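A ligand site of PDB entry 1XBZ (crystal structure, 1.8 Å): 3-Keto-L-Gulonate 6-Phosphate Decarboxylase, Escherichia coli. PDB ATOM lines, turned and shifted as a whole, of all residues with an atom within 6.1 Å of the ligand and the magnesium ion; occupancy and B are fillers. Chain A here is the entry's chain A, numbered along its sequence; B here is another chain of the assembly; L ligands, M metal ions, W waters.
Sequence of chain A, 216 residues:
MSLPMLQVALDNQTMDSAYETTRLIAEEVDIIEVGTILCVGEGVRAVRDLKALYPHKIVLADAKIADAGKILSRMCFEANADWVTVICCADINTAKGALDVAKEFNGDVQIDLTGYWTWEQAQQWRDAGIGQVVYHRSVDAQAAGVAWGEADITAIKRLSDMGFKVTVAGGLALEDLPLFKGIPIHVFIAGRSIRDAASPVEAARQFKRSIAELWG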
ATOM      1  N   GLN A   7       5.833  -8.522 -28.660  1.00  0.00           N
ATOM      2  CA  GLN A   7       4.758  -8.092 -27.733  1.00  0.00           C
ATOM      3  C   GLN A   7       5.284  -6.861 -27.064  1.00  0.00           C
ATOM      4  O   GLN A   7       6.405  -6.879 -26.524  1.00  0.00           O
ATOM      5  CB  GLN A   7       4.502  -9.187 -26.687  1.00  0.00           C
ATOM      6  CG  GLN A   7       3.607  -8.818 -25.467  1.00  0.00           C
ATOM      7  CD  GLN A   7       3.211 -10.058 -24.702  1.00  0.00           C
ATOM      8  OE1 GLN A   7       3.070 -11.124 -25.304  1.00  0.00           O
ATOM      9  NE2 GLN A   7       3.014  -9.924 -23.368  1.00  0.00           N
ATOM     10  N   ALA A   9       4.880  -4.365 -23.863  1.00  0.00           N
ATOM     11  CA  ALA A   9       4.286  -4.367 -22.525  1.00  0.00           C
ATOM     12  C   ALA A   9       3.953  -2.946 -22.210  1.00  0.00           C
ATOM     13  O   ALA A   9       4.870  -2.117 -22.132  1.00  0.00           O
ATOM     14  CB  ALA A   9       5.254  -4.896 -21.479  1.00  0.00           C
ATOM     15  N   LEU A  10       2.677  -2.677 -21.986  1.00  0.00           N
ATOM     16  CA  LEU A  10       2.237  -1.352 -21.533  1.00  0.00           C
ATOM     17  C   LEU A  10       2.220  -1.325 -20.017  1.00  0.00           C
ATOM     18  O   LEU A  10       1.191  -1.492 -19.384  1.00  0.00           O
ATOM     19  CB  LEU A  10       0.894  -0.942 -22.124  1.00  0.00           C
ATOM     20  CG  LEU A  10       0.800  -1.078 -23.644  1.00  0.00           C
ATOM     21  CD1 LEU A  10      -0.574  -0.908 -24.136  1.00  0.00           C
ATOM     22  CD2 LEU A  10       1.733   0.028 -24.255  1.00  0.00           C
ATOM     23  N   ASP A  11       3.390  -1.144 -19.450  1.00  0.00           N
ATOM     24  CA  ASP A  11       3.513  -0.975 -18.012  1.00  0.00           C
ATOM     25  C   ASP A  11       3.401   0.500 -17.671  1.00  0.00           C
ATOM     26  O   ASP A  11       4.378   1.146 -17.287  1.00  0.00           O
ATOM     27  CB  ASP A  11       4.817  -1.592 -17.492  1.00  0.00           C
ATOM     28  CG  ASP A  11       4.794  -3.104 -17.573  1.00  0.00           C
ATOM     29  OD1 ASP A  11       3.761  -3.726 -17.141  1.00  0.00           O
ATOM     30  OD2 ASP A  11       5.730  -3.739 -18.095  1.00  0.00           O
ATOM     31  N   GLU A  33       0.200  -5.871 -24.674  1.00  0.00           N
ATOM     32  CA  GLU A  33       0.041  -6.292 -23.305  1.00  0.00           C
ATOM     33  C   GLU A  33      -0.451  -5.126 -22.455  1.00  0.00           C
ATOM     34  O   GLU A  33       0.165  -4.050 -22.387  1.00  0.00           O
ATOM     35  CB  GLU A  33       1.320  -6.863 -22.719  1.00  0.00           C
ATOM     36  CG  GLU A  33       1.390  -6.780 -21.198  1.00  0.00           C
ATOM     37  CD  GLU A  33       2.699  -7.271 -20.584  1.00  0.00           C
ATOM     38  OE1 GLU A  33       3.433  -8.033 -21.228  1.00  0.00           O
ATOM     39  OE2 GLU A  33       2.947  -6.960 -19.405  1.00  0.00           O
ATOM     40  N   VAL A  34      -1.565  -5.360 -21.767  1.00  0.00           N
ATOM     41  CA  VAL A  34      -1.931  -4.536 -20.625  1.00  0.00           C
ATOM     42  C   VAL A  34      -1.076  -4.994 -19.451  1.00  0.00           C
ATOM     43  O   VAL A  34      -1.303  -6.057 -18.846  1.00  0.00           O
ATOM     44  CB  VAL A  34      -3.411  -4.719 -20.303  1.00  0.00           C
ATOM     45  CG1 VAL A  34      -3.826  -3.740 -19.179  1.00  0.00           C
ATOM     46  CG2 VAL A  34      -4.204  -4.477 -21.574  1.00  0.00           C
ATOM     47  N   GLY A  35      -0.052  -4.204 -19.122  1.00  0.00           N
ATOM     48  CA  GLY A  35       0.858  -4.580 -18.063  1.00  0.00           C
ATOM     49  C   GLY A  35       0.147  -4.667 -16.732  1.00  0.00           C
ATOM     50  O   GLY A  35      -0.887  -4.045 -16.508  1.00  0.00           O
ATOM     51  N   THR A  36       0.733  -5.388 -15.804  1.00  0.00           N
ATOM     52  CA  THR A  36       0.192  -5.459 -14.441  1.00  0.00           C
ATOM     53  C   THR A  36      -0.039  -4.069 -13.811  1.00  0.00           C
ATOM     54  O   THR A  36      -1.091  -3.837 -13.209  1.00  0.00           O
ATOM     55  CB  THR A  36       1.139  -6.281 -13.567  1.00  0.00           C
ATOM     56  OG1 THR A  36       1.489  -7.498 -14.257  1.00  0.00           O
ATOM     57  CG2 THR A  36       0.397  -6.705 -12.273  1.00  0.00           C
ATOM     58  N   LEU A  60      -3.246  -9.058 -24.366  1.00  0.00           N
ATOM     59  CA  LEU A  60      -2.865  -9.873 -23.234  1.00  0.00           C
ATOM     60  C   LEU A  60      -3.083  -9.056 -21.986  1.00  0.00           C
ATOM     61  O   LEU A  60      -2.595  -7.927 -21.892  1.00  0.00           O
ATOM     62  CB  LEU A  60      -1.397 -10.291 -23.352  1.00  0.00           C
ATOM     63  CG  LEU A  60      -0.658 -11.028 -22.204  1.00  0.00           C
ATOM     64  CD1 LEU A  60       0.003 -10.127 -21.261  1.00  0.00           C
ATOM     65  CD2 LEU A  60      -1.527 -11.996 -21.426  1.00  0.00           C
ATOM     66  N   ASP A  62      -1.988  -8.793 -18.382  1.00  0.00           N
ATOM     67  CA  ASP A  62      -0.964  -9.328 -17.502  1.00  0.00           C
ATOM     68  C   ASP A  62      -1.365  -9.215 -16.024  1.00  0.00           C
ATOM     69  O   ASP A  62      -0.705  -8.584 -15.211  1.00  0.00           O
ATOM     70  CB  ASP A  62       0.400  -8.682 -17.801  1.00  0.00           C
ATOM     71  CG  ASP A  62       1.572  -9.492 -17.249  1.00  0.00           C
ATOM     72  OD1 ASP A  62       1.381 -10.667 -16.804  1.00  0.00           O
ATOM     73  OD2 ASP A  62       2.716  -9.017 -17.191  1.00  0.00           O
ATOM     74  N   LYS A  64      -1.517 -11.597 -13.730  1.00  0.00           N
ATOM     75  CA  LYS A  64      -0.750 -12.437 -12.814  1.00  0.00           C
ATOM     76  C   LYS A  64      -1.675 -13.005 -11.732  1.00  0.00           C
ATOM     77  O   LYS A  64      -1.416 -12.904 -10.525  1.00  0.00           O
ATOM     78  CB  LYS A  64       0.422 -11.661 -12.223  1.00  0.00           C
ATOM     79  CG  LYS A  64       1.457 -11.273 -13.353  1.00  0.00           C
ATOM     80  CD  LYS A  64       2.745 -10.724 -12.825  1.00  0.00           C
ATOM     81  CE  LYS A  64       3.719 -10.488 -13.989  1.00  0.00           C
ATOM     82  NZ  LYS A  64       4.101  -9.096 -14.125  1.00  0.00           N
ATOM     83  N   ASP A 112       2.864 -17.230 -15.738  1.00  0.00           N
ATOM     84  CA  ASP A 112       3.923 -16.268 -15.688  1.00  0.00           C
ATOM     85  C   ASP A 112       4.931 -16.763 -14.680  1.00  0.00           C
ATOM     86  O   ASP A 112       4.611 -16.984 -13.504  1.00  0.00           O
ATOM     87  CB  ASP A 112       3.371 -14.879 -15.309  1.00  0.00           C
ATOM     88  CG  ASP A 112       4.432 -13.797 -15.399  1.00  0.00           C
ATOM     89  OD1 ASP A 112       5.019 -13.462 -14.361  1.00  0.00           O
ATOM     90  OD2 ASP A 112       4.745 -13.236 -16.476  1.00  0.00           O
ATOM     91  N   THR A 114       7.393 -15.562 -12.905  1.00  0.00           N
ATOM     92  CA  THR A 114       8.011 -14.507 -12.137  1.00  0.00           C
ATOM     93  C   THR A 114       8.278 -15.013 -10.736  1.00  0.00           C
ATOM     94  O   THR A 114       7.376 -15.512 -10.093  1.00  0.00           O
ATOM     95  CB  THR A 114       7.058 -13.268 -12.075  1.00  0.00           C
ATOM     96  OG1 THR A 114       7.072 -12.574 -13.336  1.00  0.00           O
ATOM     97  CG2 THR A 114       7.543 -12.228 -11.070  1.00  0.00           C
ATOM     98  N   VAL A 134       5.530 -17.847 -19.621  1.00  0.00           N
ATOM     99  CA  VAL A 134       6.332 -16.635 -19.777  1.00  0.00           C
ATOM    100  C   VAL A 134       7.559 -16.702 -18.884  1.00  0.00           C
ATOM    101  O   VAL A 134       7.497 -16.573 -17.635  1.00  0.00           O
ATOM    102  CB  VAL A 134       5.556 -15.377 -19.418  1.00  0.00           C
ATOM    103  CG1 VAL A 134       6.367 -14.167 -19.775  1.00  0.00           C
ATOM    104  CG2 VAL A 134       4.232 -15.358 -20.092  1.00  0.00           C
ATOM    105  N   HIS A 136      10.789 -15.207 -17.323  1.00  0.00           N
ATOM    106  CA  HIS A 136      11.384 -13.910 -16.953  1.00  0.00           C
ATOM    107  C   HIS A 136      12.842 -13.977 -16.483  1.00  0.00           C
ATOM    108  O   HIS A 136      13.174 -14.792 -15.620  1.00  0.00           O
ATOM    109  CB  HIS A 136      10.615 -13.251 -15.829  1.00  0.00           C
ATOM    110  CG  HIS A 136       9.245 -12.799 -16.229  1.00  0.00           C
ATOM    111  ND1 HIS A 136       8.947 -11.478 -16.503  1.00  0.00           N
ATOM    112  CD2 HIS A 136       8.092 -13.489 -16.379  1.00  0.00           C
ATOM    113  CE1 HIS A 136       7.661 -11.381 -16.800  1.00  0.00           C
ATOM    114  NE2 HIS A 136       7.114 -12.579 -16.722  1.00  0.00           N
ATOM    115  N   GLN A 142      18.954  -8.630 -14.000  1.00  0.00           N
ATOM    116  CA  GLN A 142      18.980  -7.340 -14.719  1.00  0.00           C
ATOM    117  C   GLN A 142      19.841  -6.306 -13.988  1.00  0.00           C
ATOM    118  O   GLN A 142      19.427  -5.779 -12.937  1.00  0.00           O
ATOM    119  CB  GLN A 142      17.547  -6.779 -14.879  1.00  0.00           C
ATOM    120  CG  GLN A 142      16.598  -7.625 -15.746  1.00  0.00           C
ATOM    121  CD  GLN A 142      15.278  -6.931 -16.001  1.00  0.00           C
ATOM    122  OE1 GLN A 142      15.251  -5.712 -16.272  1.00  0.00           O
ATOM    123  NE2 GLN A 142      14.173  -7.674 -15.899  1.00  0.00           N
ATOM    124  N   ALA A 169      10.998 -12.693 -21.575  1.00  0.00           N
ATOM    125  CA  ALA A 169      10.710 -11.360 -21.063  1.00  0.00           C
ATOM    126  C   ALA A 169      11.637 -10.958 -19.972  1.00  0.00           C
ATOM    127  O   ALA A 169      12.118 -11.810 -19.234  1.00  0.00           O
ATOM    128  CB  ALA A 169       9.252 -11.340 -20.546  1.00  0.00           C
ATOM    129  N   GLY A 170      11.866  -9.657 -19.824  1.00  0.00           N
ATOM    130  CA  GLY A 170      12.565  -9.126 -18.660  1.00  0.00           C
ATOM    131  C   GLY A 170      13.766  -8.291 -19.049  1.00  0.00           C
ATOM    132  O   GLY A 170      14.862  -8.827 -19.197  1.00  0.00           O
ATOM    133  N   GLY A 171      13.552  -6.981 -19.224  1.00  0.00           N
ATOM    134  CA  GLY A 171      14.565  -6.066 -19.711  1.00  0.00           C
ATOM    135  C   GLY A 171      15.150  -6.444 -21.046  1.00  0.00           C
ATOM    136  O   GLY A 171      16.317  -6.185 -21.309  1.00  0.00           O
ATOM    137  N   LEU A 172      14.359  -7.077 -21.915  1.00  0.00           N
ATOM    138  CA  LEU A 172      14.873  -7.524 -23.195  1.00  0.00           C
ATOM    139  C   LEU A 172      15.371  -6.327 -24.017  1.00  0.00           C
ATOM    140  O   LEU A 172      14.652  -5.331 -24.181  1.00  0.00           O
ATOM    141  CB  LEU A 172      13.820  -8.296 -23.964  1.00  0.00           C
ATOM    142  CG  LEU A 172      14.290  -8.965 -25.267  1.00  0.00           C
ATOM    143  CD1 LEU A 172      15.167 -10.213 -25.001  1.00  0.00           C
ATOM    144  CD2 LEU A 172      13.118  -9.309 -26.182  1.00  0.00           C
ATOM    145  N   ILE A 189       8.825 -10.351 -25.403  1.00  0.00           N
ATOM    146  CA  ILE A 189       8.288  -9.105 -24.837  1.00  0.00           C
ATOM    147  C   ILE A 189       9.328  -8.004 -24.733  1.00  0.00           C
ATOM    148  O   ILE A 189      10.429  -8.218 -24.227  1.00  0.00           O
ATOM    149  CB  ILE A 189       7.697  -9.313 -23.460  1.00  0.00           C
ATOM    150  CG1 ILE A 189       6.704 -10.464 -23.460  1.00  0.00           C
ATOM    151  CG2 ILE A 189       7.076  -7.979 -22.957  1.00  0.00           C
ATOM    152  CD1 ILE A 189       6.059 -10.753 -22.082  1.00  0.00           C
ATOM    153  N   ALA A 190       8.959  -6.810 -25.181  1.00  0.00           N
ATOM    154  CA  ALA A 190       9.686  -5.575 -24.904  1.00  0.00           C
ATOM    155  C   ALA A 190       8.778  -4.513 -24.325  1.00  0.00           C
ATOM    156  O   ALA A 190       7.787  -4.140 -24.981  1.00  0.00           O
ATOM    157  CB  ALA A 190      10.321  -5.029 -26.199  1.00  0.00           C
ATOM    158  N   GLY A 191       9.102  -4.034 -23.117  1.00  0.00           N
ATOM    159  CA  GLY A 191       8.425  -2.918 -22.468  1.00  0.00           C
ATOM    160  C   GLY A 191       9.312  -1.696 -22.613  1.00  0.00           C
ATOM    161  O   GLY A 191       9.206  -0.960 -23.587  1.00  0.00           O
ATOM    162  N   ARG A 192      10.243  -1.519 -21.700  1.00  0.00           N
ATOM    163  CA  ARG A 192      11.002  -0.283 -21.652  1.00  0.00           C
ATOM    164  C   ARG A 192      11.799  -0.065 -22.933  1.00  0.00           C
ATOM    165  O   ARG A 192      11.911   1.064 -23.390  1.00  0.00           O
ATOM    166  CB  ARG A 192      11.945  -0.263 -20.441  1.00  0.00           C
ATOM    167  CG  ARG A 192      11.229  -0.050 -19.139  1.00  0.00           C
ATOM    168  CD  ARG A 192      12.104  -0.468 -17.929  1.00  0.00           C
ATOM    169  NE  ARG A 192      12.150  -1.920 -17.857  1.00  0.00           N
ATOM    170  CZ  ARG A 192      13.022  -2.626 -17.131  1.00  0.00           C
ATOM    171  NH1 ARG A 192      12.953  -3.941 -17.153  1.00  0.00           N
ATOM    172  NH2 ARG A 192      13.940  -2.014 -16.363  1.00  0.00           N
ATOM    173  N   SER A 193      12.295  -1.146 -23.524  1.00  0.00           N
ATOM    174  CA  SER A 193      13.204  -1.050 -24.665  1.00  0.00           C
ATOM    175  C   SER A 193      12.471  -0.566 -25.926  1.00  0.00           C
ATOM    176  O   SER A 193      13.096  -0.072 -26.859  1.00  0.00           O
ATOM    177  CB  SER A 193      13.954  -2.377 -24.901  1.00  0.00           C
ATOM    178  OG  SER A 193      13.117  -3.394 -25.476  1.00  0.00           O
ATOM    179  N   ARG A 195       9.075   1.362 -25.294  1.00  0.00           N
ATOM    180  CA  ARG A 195       8.406   2.576 -24.782  1.00  0.00           C
ATOM    181  C   ARG A 195       9.340   3.744 -24.560  1.00  0.00           C
ATOM    182  O   ARG A 195       8.977   4.912 -24.816  1.00  0.00           O
ATOM    183  CB  ARG A 195       7.730   2.283 -23.461  1.00  0.00           C
ATOM    184  CG  ARG A 195       6.607   1.239 -23.554  1.00  0.00           C
ATOM    185  CD  ARG A 195       5.583   1.429 -22.415  1.00  0.00           C
ATOM    186  NE  ARG A 195       6.269   1.668 -21.156  1.00  0.00           N
ATOM    187  CZ  ARG A 195       6.808   0.725 -20.389  1.00  0.00           C
ATOM    188  NH1 ARG A 195       6.728  -0.561 -20.708  1.00  0.00           N
ATOM    189  NH2 ARG A 195       7.448   1.069 -19.290  1.00  0.00           N
ATOM    190  N   ASP B  67       5.780  -8.616  -8.687  1.00  0.00           N
ATOM    191  CA  ASP B  67       6.993  -8.022  -9.270  1.00  0.00           C
ATOM    192  C   ASP B  67       6.746  -6.537  -9.296  1.00  0.00           C
ATOM    193  O   ASP B  67       5.624  -6.094  -9.044  1.00  0.00           O
ATOM    194  CB  ASP B  67       7.175  -8.508 -10.688  1.00  0.00           C
ATOM    195  CG  ASP B  67       6.107  -7.945 -11.627  1.00  0.00           C
ATOM    196  OD1 ASP B  67       6.454  -7.158 -12.553  1.00  0.00           O
ATOM    197  OD2 ASP B  67       4.884  -8.180 -11.456  1.00  0.00           O
HETATM  198  O1  LIG L   1      11.075  -5.562 -18.631  1.00  0.00           O
HETATM  199  P1  LIG L   1      10.294  -4.841 -19.703  1.00  0.00           P
HETATM  200  O2  LIG L   1      10.234  -3.345 -19.476  1.00  0.00           O
HETATM  201  O3  LIG L   1      10.752  -5.238 -21.067  1.00  0.00           O
HETATM  202  O4  LIG L   1       8.749  -5.320 -19.546  1.00  0.00           O
HETATM  203  C1  LIG L   1       8.276  -6.609 -19.923  1.00  0.00           C
HETATM  204  C2  LIG L   1       8.030  -7.358 -18.616  1.00  0.00           C
HETATM  205  O5  LIG L   1       7.613  -8.664 -18.993  1.00  0.00           O
HETATM  206  C3  LIG L   1       6.978  -6.743 -17.710  1.00  0.00           C
HETATM  207  O6  LIG L   1       5.761  -6.398 -18.406  1.00  0.00           O
HETATM  208  C4  LIG L   1       6.775  -7.885 -16.728  1.00  0.00           C
HETATM  209  O7  LIG L   1       5.442  -8.231 -16.487  1.00  0.00           O
HETATM  210  C5  LIG L   1       7.556  -7.777 -15.482  1.00  0.00           C
HETATM  211 MG    MG M   1       4.056  -7.672 -17.899  1.00  0.00          MG
HETATM  212  O   HOH W   1      12.733  -3.824 -22.221  1.00  0.00           O
HETATM  213  O   HOH W   2      11.458  -7.632 -21.790  1.00  0.00           O
HETATM  214  O   HOH W   3       7.870  -2.313 -18.819  1.00  0.00           O
HETATM  215  O   HOH W   4       4.815  -9.135 -19.338  1.00  0.00           O
HETATM  216  O   HOH W   5       7.922 -10.094 -13.414  1.00  0.00           O
HETATM  217  O   HOH W   6       3.524  -6.285 -16.579  1.00  0.00           O
HETATM  218  O   HOH W   7      10.784  -6.455 -16.288  1.00  0.00           O
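O6 of the ligand sits close to OD2 of Asp 11 (2.7 Å). An oxygen (O7) of the ligand sits close to the side-chain amino group (NZ) of Lys 64, 2.9 Å away. O2 of the ligand sits at hydrogen-bond distance from N of Arg 192 (2.9 Å). The guanidinium group (NE) of Arg 192 lies within salt-bridge range of an oxygen (O2) of the ligand. An oxygen (O3) of the ligand is in hydrogen-bond range of the backbone NH of Gly 191 (2.9 Å). O1 of the ligand lies within hydrogen-bond range of N of Gly 171.
The side-chain carboxylate of Glu 33 is in hydrogen-bond range of the side-chain amide nitrogen of Gln 7 (2.9 Å). The backbone carbonyl oxygen (O) of Glu 33 sits at hydrogen-bond distance from the backbone NH (N) of Leu 10, at 2.9 Å. The side-chain carboxylate (OD2) of Asp 62 lies close to the side-chain amino group (NZ) of Lys 64 (3.4 Å). NH1 of Arg 192 is in hydrogen-bond range of OE1 of Gln 142 (3.0 Å). The backbone NH (N) of Ala 9 sits at hydrogen-bond distance from the backbone carbonyl oxygen (O) of Ala 190 (3.1 Å). O of Ala 9 lies within hydrogen-bond range of NH1 of Arg 195 (2.8 Å). A ring nitrogen (NE2) of His 136 lies close to the side-chain hydroxyl of Thr 114 (3.4 Å). The backbone carbonyl oxygen (O) of Gln 7 is in hydrogen-bond range of the backbone NH (N) of Ala 190.
CB of Ala 9 touches O6 of the ligand, 3.5 Å away. His 136 touches the ligand. Ala 169 touches the ligand (CB to O5, 3.5 Å). Gly 170 touches the ligand (C to O1, 3.9 Å). CG2 of Ile 189 touches C1 of the ligand, at 3.5 Å. Ala 190 touches the ligand (C to O3, 3.9 Å). OD1 of Asp 67 of chain B touches C5 of the ligand (3.2 Å). Of the 27 residues printed, 14 come within 4 Å of the ligand. The nearest printed residue that does not touch the ligand is Leu 172 (4.1 Å).
Two residues have an atom within 4 Å of the magnesium ion: Glu 33 and Asp 62. The nearest printed residue that does not touch the magnesium ion is Asp 11 (4.03 Å).
Water W6 is bound to the magnesium ion (2.0 Å). OE2 of Glu 33 is bound to the magnesium ion, 2.0 Å away. The magnesium ion is bound by OD2 of Asp 62 (2.0 Å). An oxygen (O7) of the ligand binds the magnesium ion (2.1 Å). The magnesium ion is bound by O6 of the ligand (2.2 Å). The magnesium ion is bound by water W4. The magnesium ion has six donor atoms within binding distance.
Water W6 bridges the side-chain carboxylate (OD1) of Asp 11 (2.6 Å) and the backbone NH (N) of Thr 36 (3.0 Å). Water W4 lies within hydrogen-bond range of the side-chain carboxylate of Glu 33 (2.6 Å) and an oxygen (O5) of the ligand (2.9 Å). Water W7 bridges O1 of the ligand (2.5 Å) and NH1 of Arg 192 (3.4 Å). Water W3 lies within hydrogen-bond range of O2 of the ligand, OD2 of Asp 11 and NH1 of Arg 195. Water W1 lies within hydrogen-bond range of O3 of the ligand, N of Ser 193, O of Leu 172 and N of Arg 192. Water W5 lies within hydrogen-bond range of the side-chain hydroxyl of Thr 114 (2.6 Å) and the side-chain carboxylate of Asp 67 of chain B (3.4 Å).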
